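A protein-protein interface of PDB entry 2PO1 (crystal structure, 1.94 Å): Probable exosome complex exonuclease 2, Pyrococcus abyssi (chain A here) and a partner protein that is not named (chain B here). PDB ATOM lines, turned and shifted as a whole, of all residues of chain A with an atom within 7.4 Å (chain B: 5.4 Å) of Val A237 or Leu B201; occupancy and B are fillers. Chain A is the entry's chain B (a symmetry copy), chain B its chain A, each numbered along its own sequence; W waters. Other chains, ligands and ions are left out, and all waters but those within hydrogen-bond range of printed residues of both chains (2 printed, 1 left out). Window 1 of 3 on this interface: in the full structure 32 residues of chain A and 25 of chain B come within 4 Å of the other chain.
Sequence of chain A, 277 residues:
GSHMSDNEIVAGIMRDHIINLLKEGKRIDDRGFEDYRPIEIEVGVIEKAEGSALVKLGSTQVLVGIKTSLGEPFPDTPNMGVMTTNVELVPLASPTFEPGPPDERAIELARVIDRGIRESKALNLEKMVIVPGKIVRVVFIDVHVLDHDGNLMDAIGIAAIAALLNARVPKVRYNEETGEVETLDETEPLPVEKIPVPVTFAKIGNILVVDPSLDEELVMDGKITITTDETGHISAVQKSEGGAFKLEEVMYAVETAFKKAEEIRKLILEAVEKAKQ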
ATOM      1  N   VAL A 112      15.336  12.642  39.042  1.00  0.00           N
ATOM      2  CA  VAL A 112      14.930  12.887  37.673  1.00  0.00           C
ATOM      3  C   VAL A 112      13.416  12.763  37.592  1.00  0.00           C
ATOM      4  O   VAL A 112      12.790  13.481  36.862  1.00  0.00           O
ATOM      5  CB  VAL A 112      15.532  11.852  36.753  1.00  0.00           C
ATOM      6  CG1 VAL A 112      14.884  11.877  35.395  1.00  0.00           C
ATOM      7  CG2 VAL A 112      17.026  12.002  36.696  1.00  0.00           C
ATOM      8  N   ARG A 115      11.882  15.696  39.234  1.00  0.00           N
ATOM      9  CA  ARG A 115      12.008  16.876  38.411  1.00  0.00           C
ATOM     10  C   ARG A 115      10.941  16.870  37.379  1.00  0.00           C
ATOM     11  O   ARG A 115      10.332  17.913  37.139  1.00  0.00           O
ATOM     12  CB  ARG A 115      13.369  16.975  37.764  1.00  0.00           C
ATOM     13  CG  ARG A 115      14.347  17.380  38.816  1.00  0.00           C
ATOM     14  CD  ARG A 115      15.544  17.991  38.170  1.00  0.00           C
ATOM     15  NE  ARG A 115      16.236  17.060  37.309  1.00  0.00           N
ATOM     16  CZ  ARG A 115      17.256  16.301  37.704  1.00  0.00           C
ATOM     17  NH1 ARG A 115      17.832  15.516  36.829  1.00  0.00           N
ATOM     18  NH2 ARG A 115      17.701  16.330  38.964  1.00  0.00           N
ATOM     19  N   GLY A 116      10.680  15.694  36.814  1.00  0.00           N
ATOM     20  CA  GLY A 116       9.669  15.566  35.726  1.00  0.00           C
ATOM     21  C   GLY A 116       8.325  16.057  36.209  1.00  0.00           C
ATOM     22  O   GLY A 116       7.572  16.663  35.465  1.00  0.00           O
ATOM     23  N   LYS A 223      22.612   6.331  27.976  1.00  0.00           N
ATOM     24  CA  LYS A 223      21.175   6.275  28.102  1.00  0.00           C
ATOM     25  C   LYS A 223      20.714   7.684  28.209  1.00  0.00           C
ATOM     26  O   LYS A 223      21.476   8.537  28.620  1.00  0.00           O
ATOM     27  CB  LYS A 223      20.860   5.511  29.371  1.00  0.00           C
ATOM     28  CG  LYS A 223      19.490   5.657  29.910  1.00  0.00           C
ATOM     29  CD  LYS A 223      19.386   4.775  31.137  1.00  0.00           C
ATOM     30  CE  LYS A 223      18.766   3.478  30.735  1.00  0.00           C
ATOM     31  NZ  LYS A 223      18.404   2.579  31.842  1.00  0.00           N
ATOM     32  N   ILE A 224      19.499   7.950  27.758  1.00  0.00           N
ATOM     33  CA  ILE A 224      18.975   9.294  27.851  1.00  0.00           C
ATOM     34  C   ILE A 224      17.517   9.169  28.129  1.00  0.00           C
ATOM     35  O   ILE A 224      16.838   8.308  27.566  1.00  0.00           O
ATOM     36  CB  ILE A 224      19.240  10.182  26.524  1.00  0.00           C
ATOM     37  CG1 ILE A 224      18.839  11.644  26.789  1.00  0.00           C
ATOM     38  CG2 ILE A 224      18.511   9.613  25.336  1.00  0.00           C
ATOM     39  CD1 ILE A 224      19.368  12.644  25.784  1.00  0.00           C
ATOM     40  N   THR A 225      17.054   9.989  29.068  1.00  0.00           N
ATOM     41  CA  THR A 225      15.653   9.985  29.441  1.00  0.00           C
ATOM     42  C   THR A 225      15.118  11.346  29.117  1.00  0.00           C
ATOM     43  O   THR A 225      15.762  12.348  29.435  1.00  0.00           O
ATOM     44  CB  THR A 225      15.486   9.744  30.940  1.00  0.00           C
ATOM     45  OG1 THR A 225      15.816   8.384  31.249  1.00  0.00           O
ATOM     46  CG2 THR A 225      14.069  10.042  31.349  1.00  0.00           C
ATOM     47  N   ILE A 226      14.004  11.355  28.380  1.00  0.00           N
ATOM     48  CA  ILE A 226      13.226  12.550  28.065  1.00  0.00           C
ATOM     49  C   ILE A 226      11.855  12.423  28.701  1.00  0.00           C
ATOM     50  O   ILE A 226      11.109  11.503  28.379  1.00  0.00           O
ATOM     51  CB  ILE A 226      12.942  12.682  26.509  1.00  0.00           C
ATOM     52  CG1 ILE A 226      14.191  12.345  25.673  1.00  0.00           C
ATOM     53  CG2 ILE A 226      12.380  14.030  26.201  1.00  0.00           C
ATOM     54  CD1 ILE A 226      15.375  13.295  25.969  1.00  0.00           C
ATOM     55  N   THR A 227      11.500  13.363  29.559  1.00  0.00           N
ATOM     56  CA  THR A 227      10.220  13.364  30.196  1.00  0.00           C
ATOM     57  C   THR A 227       9.369  14.491  29.667  1.00  0.00           C
ATOM     58  O   THR A 227       9.787  15.648  29.680  1.00  0.00           O
ATOM     59  CB  THR A 227      10.401  13.582  31.717  1.00  0.00           C
ATOM     60  OG1 THR A 227      11.250  12.569  32.211  1.00  0.00           O
ATOM     61  CG2 THR A 227       9.054  13.555  32.437  1.00  0.00           C
ATOM     62  N   THR A 228       8.180  14.158  29.183  1.00  0.00           N
ATOM     63  CA  THR A 228       7.357  15.111  28.503  1.00  0.00           C
ATOM     64  C   THR A 228       5.937  14.984  29.019  1.00  0.00           C
ATOM     65  O   THR A 228       5.546  13.904  29.469  1.00  0.00           O
ATOM     66  CB  THR A 228       7.373  14.895  26.976  1.00  0.00           C
ATOM     67  OG1 THR A 228       6.847  13.607  26.690  1.00  0.00           O
ATOM     68  CG2 THR A 228       8.786  14.972  26.460  1.00  0.00           C
ATOM     69  N   ILE A 234       8.821  19.539  27.659  1.00  0.00           N
ATOM     70  CA  ILE A 234       9.780  18.660  28.256  1.00  0.00           C
ATOM     71  C   ILE A 234       9.973  19.169  29.660  1.00  0.00           C
ATOM     72  O   ILE A 234      10.226  20.351  29.876  1.00  0.00           O
ATOM     73  CB  ILE A 234      11.129  18.604  27.486  1.00  0.00           C
ATOM     74  CG1 ILE A 234      10.922  18.364  25.979  1.00  0.00           C
ATOM     75  CG2 ILE A 234      11.996  17.524  28.034  1.00  0.00           C
ATOM     76  CD1 ILE A 234      12.009  18.984  25.152  1.00  0.00           C
ATOM     77  N   SER A 235       9.828  18.294  30.638  1.00  0.00           N
ATOM     78  CA  SER A 235      10.014  18.732  32.029  1.00  0.00           C
ATOM     79  C   SER A 235      11.251  18.134  32.643  1.00  0.00           C
ATOM     80  O   SER A 235      11.666  18.556  33.713  1.00  0.00           O
ATOM     81  CB  SER A 235       8.781  18.394  32.880  1.00  0.00           C
ATOM     82  OG  SER A 235       8.485  17.016  32.785  1.00  0.00           O
ATOM     83  N   ALA A 236      11.903  17.179  31.947  1.00  0.00           N
ATOM     84  CA  ALA A 236      13.218  16.725  32.389  1.00  0.00           C
ATOM     85  C   ALA A 236      13.912  16.013  31.279  1.00  0.00           C
ATOM     86  O   ALA A 236      13.285  15.357  30.420  1.00  0.00           O
ATOM     87  CB  ALA A 236      13.079  15.729  33.513  1.00  0.00           C
ATOM     88  N   VAL A 237      15.225  16.110  31.319  1.00  0.00           N
ATOM     89  CA  VAL A 237      16.086  15.322  30.440  1.00  0.00           C
ATOM     90  C   VAL A 237      17.238  14.928  31.269  1.00  0.00           C
ATOM     91  O   VAL A 237      17.705  15.734  32.067  1.00  0.00           O
ATOM     92  CB  VAL A 237      16.626  16.153  29.262  1.00  0.00           C
ATOM     93  CG1 VAL A 237      17.629  15.308  28.406  1.00  0.00           C
ATOM     94  CG2 VAL A 237      15.469  16.584  28.386  1.00  0.00           C
ATOM     95  N   GLN A 238      17.690  13.691  31.079  1.00  0.00           N
ATOM     96  CA  GLN A 238      18.820  13.180  31.767  1.00  0.00           C
ATOM     97  C   GLN A 238      19.472  12.124  30.893  1.00  0.00           C
ATOM     98  O   GLN A 238      18.991  10.989  30.766  1.00  0.00           O
ATOM     99  CB  GLN A 238      18.399  12.562  33.117  1.00  0.00           C
ATOM    100  CG  GLN A 238      19.550  12.149  33.908  1.00  0.00           C
ATOM    101  CD  GLN A 238      19.934  13.129  34.970  1.00  0.00           C
ATOM    102  OE1 GLN A 238      19.547  14.299  34.945  1.00  0.00           O
ATOM    103  NE2 GLN A 238      20.680  12.636  35.981  1.00  0.00           N
ATOM    104  N   LYS A 239      20.579  12.527  30.292  1.00  0.00           N
ATOM    105  CA  LYS A 239      21.549  11.559  29.807  1.00  0.00           C
ATOM    106  C   LYS A 239      22.126  10.974  31.102  1.00  0.00           C
ATOM    107  O   LYS A 239      22.526  11.747  32.012  1.00  0.00           O
ATOM    108  CB  LYS A 239      22.633  12.264  29.012  1.00  0.00           C
ATOM    109  CG  LYS A 239      23.610  11.304  28.370  1.00  0.00           C
ATOM    110  CD  LYS A 239      24.809  11.071  29.245  1.00  0.00           C
ATOM    111  CE  LYS A 239      25.821  10.174  28.510  1.00  0.00           C
ATOM    112  NZ  LYS A 239      27.131  10.188  29.236  1.00  0.00           N
ATOM    113  N   SER A 240      22.123   9.629  31.207  1.00  0.00           N
ATOM    114  CA  SER A 240      22.641   8.900  32.335  1.00  0.00           C
ATOM    115  C   SER A 240      23.662   7.831  31.891  1.00  0.00           C
ATOM    116  O   SER A 240      23.710   7.435  30.732  1.00  0.00           O
ATOM    117  CB  SER A 240      21.533   8.271  33.177  1.00  0.00           C
ATOM    118  OG  SER A 240      20.778   7.348  32.437  1.00  0.00           O
ATOM    119  N   PHE A 245      26.028  11.111  23.131  1.00  0.00           N
ATOM    120  CA  PHE A 245      24.970  11.151  22.153  1.00  0.00           C
ATOM    121  C   PHE A 245      25.300  12.244  21.187  1.00  0.00           C
ATOM    122  O   PHE A 245      25.954  13.220  21.548  1.00  0.00           O
ATOM    123  CB  PHE A 245      23.653  11.431  22.838  1.00  0.00           C
ATOM    124  CG  PHE A 245      23.150  10.278  23.645  1.00  0.00           C
ATOM    125  CD1 PHE A 245      22.177   9.444  23.129  1.00  0.00           C
ATOM    126  CD2 PHE A 245      23.659  10.024  24.909  1.00  0.00           C
ATOM    127  CE1 PHE A 245      21.687   8.395  23.832  1.00  0.00           C
ATOM    128  CE2 PHE A 245      23.172   8.948  25.650  1.00  0.00           C
ATOM    129  CZ  PHE A 245      22.167   8.112  25.095  1.00  0.00           C
ATOM    130  N   LYS A 246      24.848  12.074  19.956  1.00  0.00           N
ATOM    131  CA  LYS A 246      24.920  13.101  18.961  1.00  0.00           C
ATOM    132  C   LYS A 246      23.705  13.985  19.171  1.00  0.00           C
ATOM    133  O   LYS A 246      22.680  13.524  19.691  1.00  0.00           O
ATOM    134  CB  LYS A 246      24.868  12.488  17.555  1.00  0.00           C
ATOM    135  CG  LYS A 246      26.050  11.604  17.202  1.00  0.00           C
ATOM    136  CD  LYS A 246      27.331  12.393  17.345  1.00  0.00           C
ATOM    137  CE  LYS A 246      28.497  11.651  16.739  1.00  0.00           C
ATOM    138  NZ  LYS A 246      29.696  12.434  17.039  1.00  0.00           N
ATOM    139  N   LEU A 247      23.829  15.244  18.785  1.00  0.00           N
ATOM    140  CA  LEU A 247      22.722  16.199  18.877  1.00  0.00           C
ATOM    141  C   LEU A 247      21.467  15.662  18.122  1.00  0.00           C
ATOM    142  O   LEU A 247      20.327  15.815  18.577  1.00  0.00           O
ATOM    143  CB  LEU A 247      23.155  17.550  18.269  1.00  0.00           C
ATOM    144  CG  LEU A 247      22.290  18.826  18.352  1.00  0.00           C
ATOM    145  CD1 LEU A 247      21.625  19.128  17.079  1.00  0.00           C
ATOM    146  CD2 LEU A 247      21.289  18.795  19.501  1.00  0.00           C
ATOM    147  N   VAL A 250      19.719  13.022  20.298  1.00  0.00           N
ATOM    148  CA  VAL A 250      18.854  13.736  21.250  1.00  0.00           C
ATOM    149  C   VAL A 250      17.538  14.224  20.648  1.00  0.00           C
ATOM    150  O   VAL A 250      16.457  13.947  21.168  1.00  0.00           O
ATOM    151  CB  VAL A 250      19.622  14.909  21.853  1.00  0.00           C
ATOM    152  CG1 VAL A 250      18.702  15.819  22.714  1.00  0.00           C
ATOM    153  CG2 VAL A 250      20.784  14.347  22.627  1.00  0.00           C
ATOM    154  N   MET A 251      17.648  14.967  19.556  1.00  0.00           N
ATOM    155  CA  MET A 251      16.486  15.423  18.824  1.00  0.00           C
ATOM    156  C   MET A 251      15.527  14.257  18.511  1.00  0.00           C
ATOM    157  O   MET A 251      14.343  14.329  18.769  1.00  0.00           O
ATOM    158  CB  MET A 251      16.943  16.082  17.530  1.00  0.00           C
ATOM    159  CG  MET A 251      17.811  17.324  17.727  1.00  0.00           C
ATOM    160  SD  MET A 251      18.531  18.062  16.196  1.00  0.00           S
ATOM    161  CE  MET A 251      17.126  18.188  15.075  1.00  0.00           C
ATOM    162  N   VAL A 254      13.925  13.130  21.699  1.00  0.00           N
ATOM    163  CA  VAL A 254      12.909  14.046  22.232  1.00  0.00           C
ATOM    164  C   VAL A 254      11.621  13.761  21.496  1.00  0.00           C
ATOM    165  O   VAL A 254      10.546  13.524  22.080  1.00  0.00           O
ATOM    166  CB  VAL A 254      13.295  15.524  21.998  1.00  0.00           C
ATOM    167  CG1 VAL A 254      12.121  16.377  22.328  1.00  0.00           C
ATOM    168  CG2 VAL A 254      14.472  15.926  22.906  1.00  0.00           C
ATOM    169  N   VAL B 187      19.917  24.029  31.336  1.00  0.00           N
ATOM    170  CA  VAL B 187      20.330  22.948  30.413  1.00  0.00           C
ATOM    171  C   VAL B 187      21.851  22.919  30.339  1.00  0.00           C
ATOM    172  O   VAL B 187      22.473  23.579  29.428  1.00  0.00           O
ATOM    173  CB  VAL B 187      19.768  23.141  28.962  1.00  0.00           C
ATOM    174  CG1 VAL B 187      20.085  21.945  28.102  1.00  0.00           C
ATOM    175  CG2 VAL B 187      18.288  23.323  28.994  1.00  0.00           C
ATOM    176  N   PRO B 188      22.452  22.180  31.269  1.00  0.00           N
ATOM    177  CA  PRO B 188      23.853  21.912  31.182  1.00  0.00           C
ATOM    178  C   PRO B 188      24.146  20.854  30.116  1.00  0.00           C
ATOM    179  O   PRO B 188      23.412  19.873  29.968  1.00  0.00           O
ATOM    180  CB  PRO B 188      24.183  21.338  32.569  1.00  0.00           C
ATOM    181  CG  PRO B 188      22.995  20.855  33.112  1.00  0.00           C
ATOM    182  CD  PRO B 188      21.854  21.572  32.498  1.00  0.00           C
ATOM    183  N   VAL B 189      25.254  21.039  29.401  1.00  0.00           N
ATOM    184  CA  VAL B 189      25.649  20.026  28.442  1.00  0.00           C
ATOM    185  C   VAL B 189      27.112  19.903  28.638  1.00  0.00           C
ATOM    186  O   VAL B 189      27.813  20.894  28.880  1.00  0.00           O
ATOM    187  CB  VAL B 189      25.362  20.521  26.995  1.00  0.00           C
ATOM    188  CG1 VAL B 189      25.689  19.504  25.948  1.00  0.00           C
ATOM    189  CG2 VAL B 189      23.932  20.915  26.854  1.00  0.00           C
ATOM    190  N   ALA B 190      27.607  18.688  28.497  1.00  0.00           N
ATOM    191  CA  ALA B 190      29.038  18.523  28.311  1.00  0.00           C
ATOM    192  C   ALA B 190      29.233  17.829  27.018  1.00  0.00           C
ATOM    193  O   ALA B 190      28.423  16.989  26.618  1.00  0.00           O
ATOM    194  CB  ALA B 190      29.667  17.730  29.496  1.00  0.00           C
ATOM    195  N   ILE B 198      27.984  14.303  22.970  1.00  0.00           N
ATOM    196  CA  ILE B 198      27.414  14.882  24.162  1.00  0.00           C
ATOM    197  C   ILE B 198      27.513  13.911  25.312  1.00  0.00           C
ATOM    198  O   ILE B 198      26.847  12.890  25.343  1.00  0.00           O
ATOM    199  CB  ILE B 198      25.964  15.358  23.946  1.00  0.00           C
ATOM    200  CG1 ILE B 198      25.894  16.412  22.820  1.00  0.00           C
ATOM    201  CG2 ILE B 198      25.349  15.826  25.275  1.00  0.00           C
ATOM    202  CD1 ILE B 198      24.524  16.622  22.280  1.00  0.00           C
ATOM    203  N   THR B 199      28.347  14.227  26.287  1.00  0.00           N
ATOM    204  CA  THR B 199      28.505  13.285  27.419  1.00  0.00           C
ATOM    205  C   THR B 199      27.745  13.658  28.613  1.00  0.00           C
ATOM    206  O   THR B 199      27.595  12.843  29.548  1.00  0.00           O
ATOM    207  CB  THR B 199      29.950  13.120  27.791  1.00  0.00           C
ATOM    208  OG1 THR B 199      30.425  14.374  28.272  1.00  0.00           O
ATOM    209  CG2 THR B 199      30.710  12.711  26.523  1.00  0.00           C
ATOM    210  N   LEU B 200      27.240  14.882  28.643  1.00  0.00           N
ATOM    211  CA  LEU B 200      26.307  15.217  29.722  1.00  0.00           C
ATOM    212  C   LEU B 200      25.183  15.974  29.137  1.00  0.00           C
ATOM    213  O   LEU B 200      25.418  16.908  28.363  1.00  0.00           O
ATOM    214  CB  LEU B 200      26.934  16.045  30.830  1.00  0.00           C
ATOM    215  CG  LEU B 200      26.040  16.482  31.986  1.00  0.00           C
ATOM    216  CD1 LEU B 200      26.741  16.434  33.304  1.00  0.00           C
ATOM    217  CD2 LEU B 200      25.431  17.858  31.796  1.00  0.00           C
ATOM    218  N   LEU B 201      23.958  15.597  29.500  1.00  0.00           N
ATOM    219  CA  LEU B 201      22.829  16.461  29.067  1.00  0.00           C
ATOM    220  C   LEU B 201      21.733  16.387  30.077  1.00  0.00           C
ATOM    221  O   LEU B 201      21.195  15.351  30.308  1.00  0.00           O
ATOM    222  CB  LEU B 201      22.258  16.067  27.706  1.00  0.00           C
ATOM    223  CG  LEU B 201      21.758  17.145  26.717  1.00  0.00           C
ATOM    224  CD1 LEU B 201      20.812  16.541  25.669  1.00  0.00           C
ATOM    225  CD2 LEU B 201      21.086  18.301  27.412  1.00  0.00           C
ATOM    226  N   GLN B 202      21.383  17.529  30.637  1.00  0.00           N
ATOM    227  CA  GLN B 202      20.360  17.571  31.630  1.00  0.00           C
ATOM    228  C   GLN B 202      19.530  18.768  31.298  1.00  0.00           C
ATOM    229  O   GLN B 202      20.005  19.715  30.671  1.00  0.00           O
ATOM    230  CB  GLN B 202      20.927  17.706  33.019  1.00  0.00           C
ATOM    231  CG  GLN B 202      21.861  16.605  33.375  1.00  0.00           C
ATOM    232  CD  GLN B 202      22.241  16.609  34.759  1.00  0.00           C
ATOM    233  OE1 GLN B 202      23.188  17.304  35.152  1.00  0.00           O
ATOM    234  NE2 GLN B 202      21.527  15.839  35.564  1.00  0.00           N
ATOM    235  N   MET B 203      18.284  18.691  31.717  1.00  0.00           N
ATOM    236  CA  MET B 203      17.365  19.789  31.590  1.00  0.00           C
ATOM    237  C   MET B 203      16.478  19.790  32.821  1.00  0.00           C
ATOM    238  O   MET B 203      15.815  18.810  33.137  1.00  0.00           O
ATOM    239  CB  MET B 203      16.557  19.656  30.309  1.00  0.00           C
ATOM    240  CG  MET B 203      15.755  20.887  29.955  1.00  0.00           C
ATOM    241  SD  MET B 203      14.263  21.009  30.914  1.00  0.00           S
ATOM    242  CE  MET B 203      13.124  20.099  29.944  1.00  0.00           C
ATOM    243  N   PHE B 212      14.199  23.498  23.976  1.00  0.00           N
ATOM    244  CA  PHE B 212      15.208  22.599  24.509  1.00  0.00           C
ATOM    245  C   PHE B 212      16.375  22.431  23.559  1.00  0.00           C
ATOM    246  O   PHE B 212      17.529  22.614  23.936  1.00  0.00           O
ATOM    247  CB  PHE B 212      14.599  21.231  24.808  1.00  0.00           C
ATOM    248  CG  PHE B 212      15.622  20.213  25.222  1.00  0.00           C
ATOM    249  CD1 PHE B 212      15.834  19.080  24.456  1.00  0.00           C
ATOM    250  CD2 PHE B 212      16.401  20.402  26.372  1.00  0.00           C
ATOM    251  CE1 PHE B 212      16.753  18.162  24.821  1.00  0.00           C
ATOM    252  CE2 PHE B 212      17.353  19.460  26.744  1.00  0.00           C
ATOM    253  CZ  PHE B 212      17.521  18.351  25.963  1.00  0.00           C
ATOM    254  N   VAL B 216      20.330  23.417  24.010  1.00  0.00           N
ATOM    255  CA  VAL B 216      21.440  22.455  23.821  1.00  0.00           C
ATOM    256  C   VAL B 216      22.452  22.980  22.793  1.00  0.00           C
ATOM    257  O   VAL B 216      23.662  23.064  23.085  1.00  0.00           O
ATOM    258  CB  VAL B 216      20.948  21.020  23.466  1.00  0.00           C
ATOM    259  CG1 VAL B 216      22.134  20.060  23.305  1.00  0.00           C
ATOM    260  CG2 VAL B 216      20.083  20.468  24.597  1.00  0.00           C
HETATM  261  O   HOH W   1      23.894  13.868  31.735  1.00  0.00           O
HETATM  262  O   HOH W   2      13.509  19.548  35.048  1.00  0.00           O
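Of the printed residues of chain B, Ser A235 touches Met B203 (3.8 Å). Of the printed residues of chain B, Ala A236 touches Met B203. Val A237 touches just these residues of chain B: Leu B201 (3.9 Å), Gln B202 (3.3 Å), Met B203 (3.0 Å) and Phe B212 (3.6 Å). Ser A240 touches none of the printed residues of chain B. Of the printed residues of chain B, Phe A245 touches Ile B198. Of the printed residues of chain B, Val A254 touches Phe B212 (3.7 Å). Printed residues of chain A within 4 Å of Leu B201: Val A237 (3.9 Å), Gln A238 (3.5 Å), Lys A239 (2.9 Å) and Val A250 (3.7 Å). Printed residues of chain A within 4 Å of Gln B202: Arg A115 (3.9 Å), Val A237 (3.3 Å) and Gln A238 (2.6 Å). The nearest residue of chain A that does not touch Leu B201 is Ile A224 (4.2 Å).
The backbone NH (N) of Thr B199 is in hydrogen-bond range of the backbone carbonyl oxygen (O) of Ala B190. NH1 of Arg A115 sits at hydrogen-bond distance from OE1 of Gln A238 (2.8 Å). O of Gly A116 is in hydrogen-bond range of OG of Ser A235 (2.9 Å). N of Thr A225 is in hydrogen-bond range of O of Gln A238 (2.8 Å). N of Ser A235 is in hydrogen-bond range of O of Thr A227, 2.8 Å away. N of Thr A227 lies within hydrogen-bond range of O of Ala A236, at 2.8 Å.
Of the 22 printed residues of chain A, 11 touch a printed residue of chain B. Hydrophobic or aromatic side chains of chain A within 4 Å of the printed part of chain B: Ile A234, Val A237, Val A250 and Val A254. Of the 12 printed residues of chain B, 6 touch a printed residue of chain A. Printed residues of chain B that touch a printed residue of chain A: Ile B198, Thr B199, Leu B201, Gln B202, Met B203 and Phe B212. Hydrophobic or aromatic side chains of chain B within 4 Å of the printed part of chain A: Ile B198, Leu B201, Met B203 and Phe B212. Among the printed residues, 18 pairs touch across the chains.
Water W2 lies within hydrogen-bond range of O of Ser A235 (2.5 Å) and O of Met B203 (3.1 Å). Water W1 lies within hydrogen-bond range of O of Lys A239 (2.5 Å) and N of Leu B201 (2.8 Å).
NE2 of Gln B202 touches NH1 of Arg A115, at 3.9 Å. Phe B212 touches Ile A234. Ser A235 touches Met B203 (N to CE, 3.8 Å). Ala A236 touches Met B203 (CA to O, 3.4 Å). Val A237 touches Leu B201 (O to O, 3.9 Å). O of Val A237 touches CA of Gln B202 (3.3 Å). CZ of Phe B212 touches CG2 of Val A237, at 3.6 Å. CA of Gln A238 touches O of Leu B201 (3.5 Å). CD1 of Ile B198 touches N of Leu A247, at 3.8 Å. Val A250 touches Leu B201 (CG1 to CD1, 3.7 Å).
N of Ile B198 is in hydrogen-bond range of O of Phe A245 (2.7 Å). The backbone carbonyl oxygen (O) of Thr B199 is in hydrogen-bond range of the side-chain amino group (NZ) of Lys A239, at 2.7 Å. The backbone carbonyl oxygen (O) of Leu B201 is in hydrogen-bond range of the backbone NH (N) of Lys A239, 2.9 Å away. The side-chain amide nitrogen of Gln B202 lies within hydrogen-bond range of the side-chain amide oxygen of Gln A238 (2.6 Å). The backbone NH (N) of Met B203 lies within hydrogen-bond range of the backbone carbonyl oxygen (O) of Val A237, at 3.0 Å.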
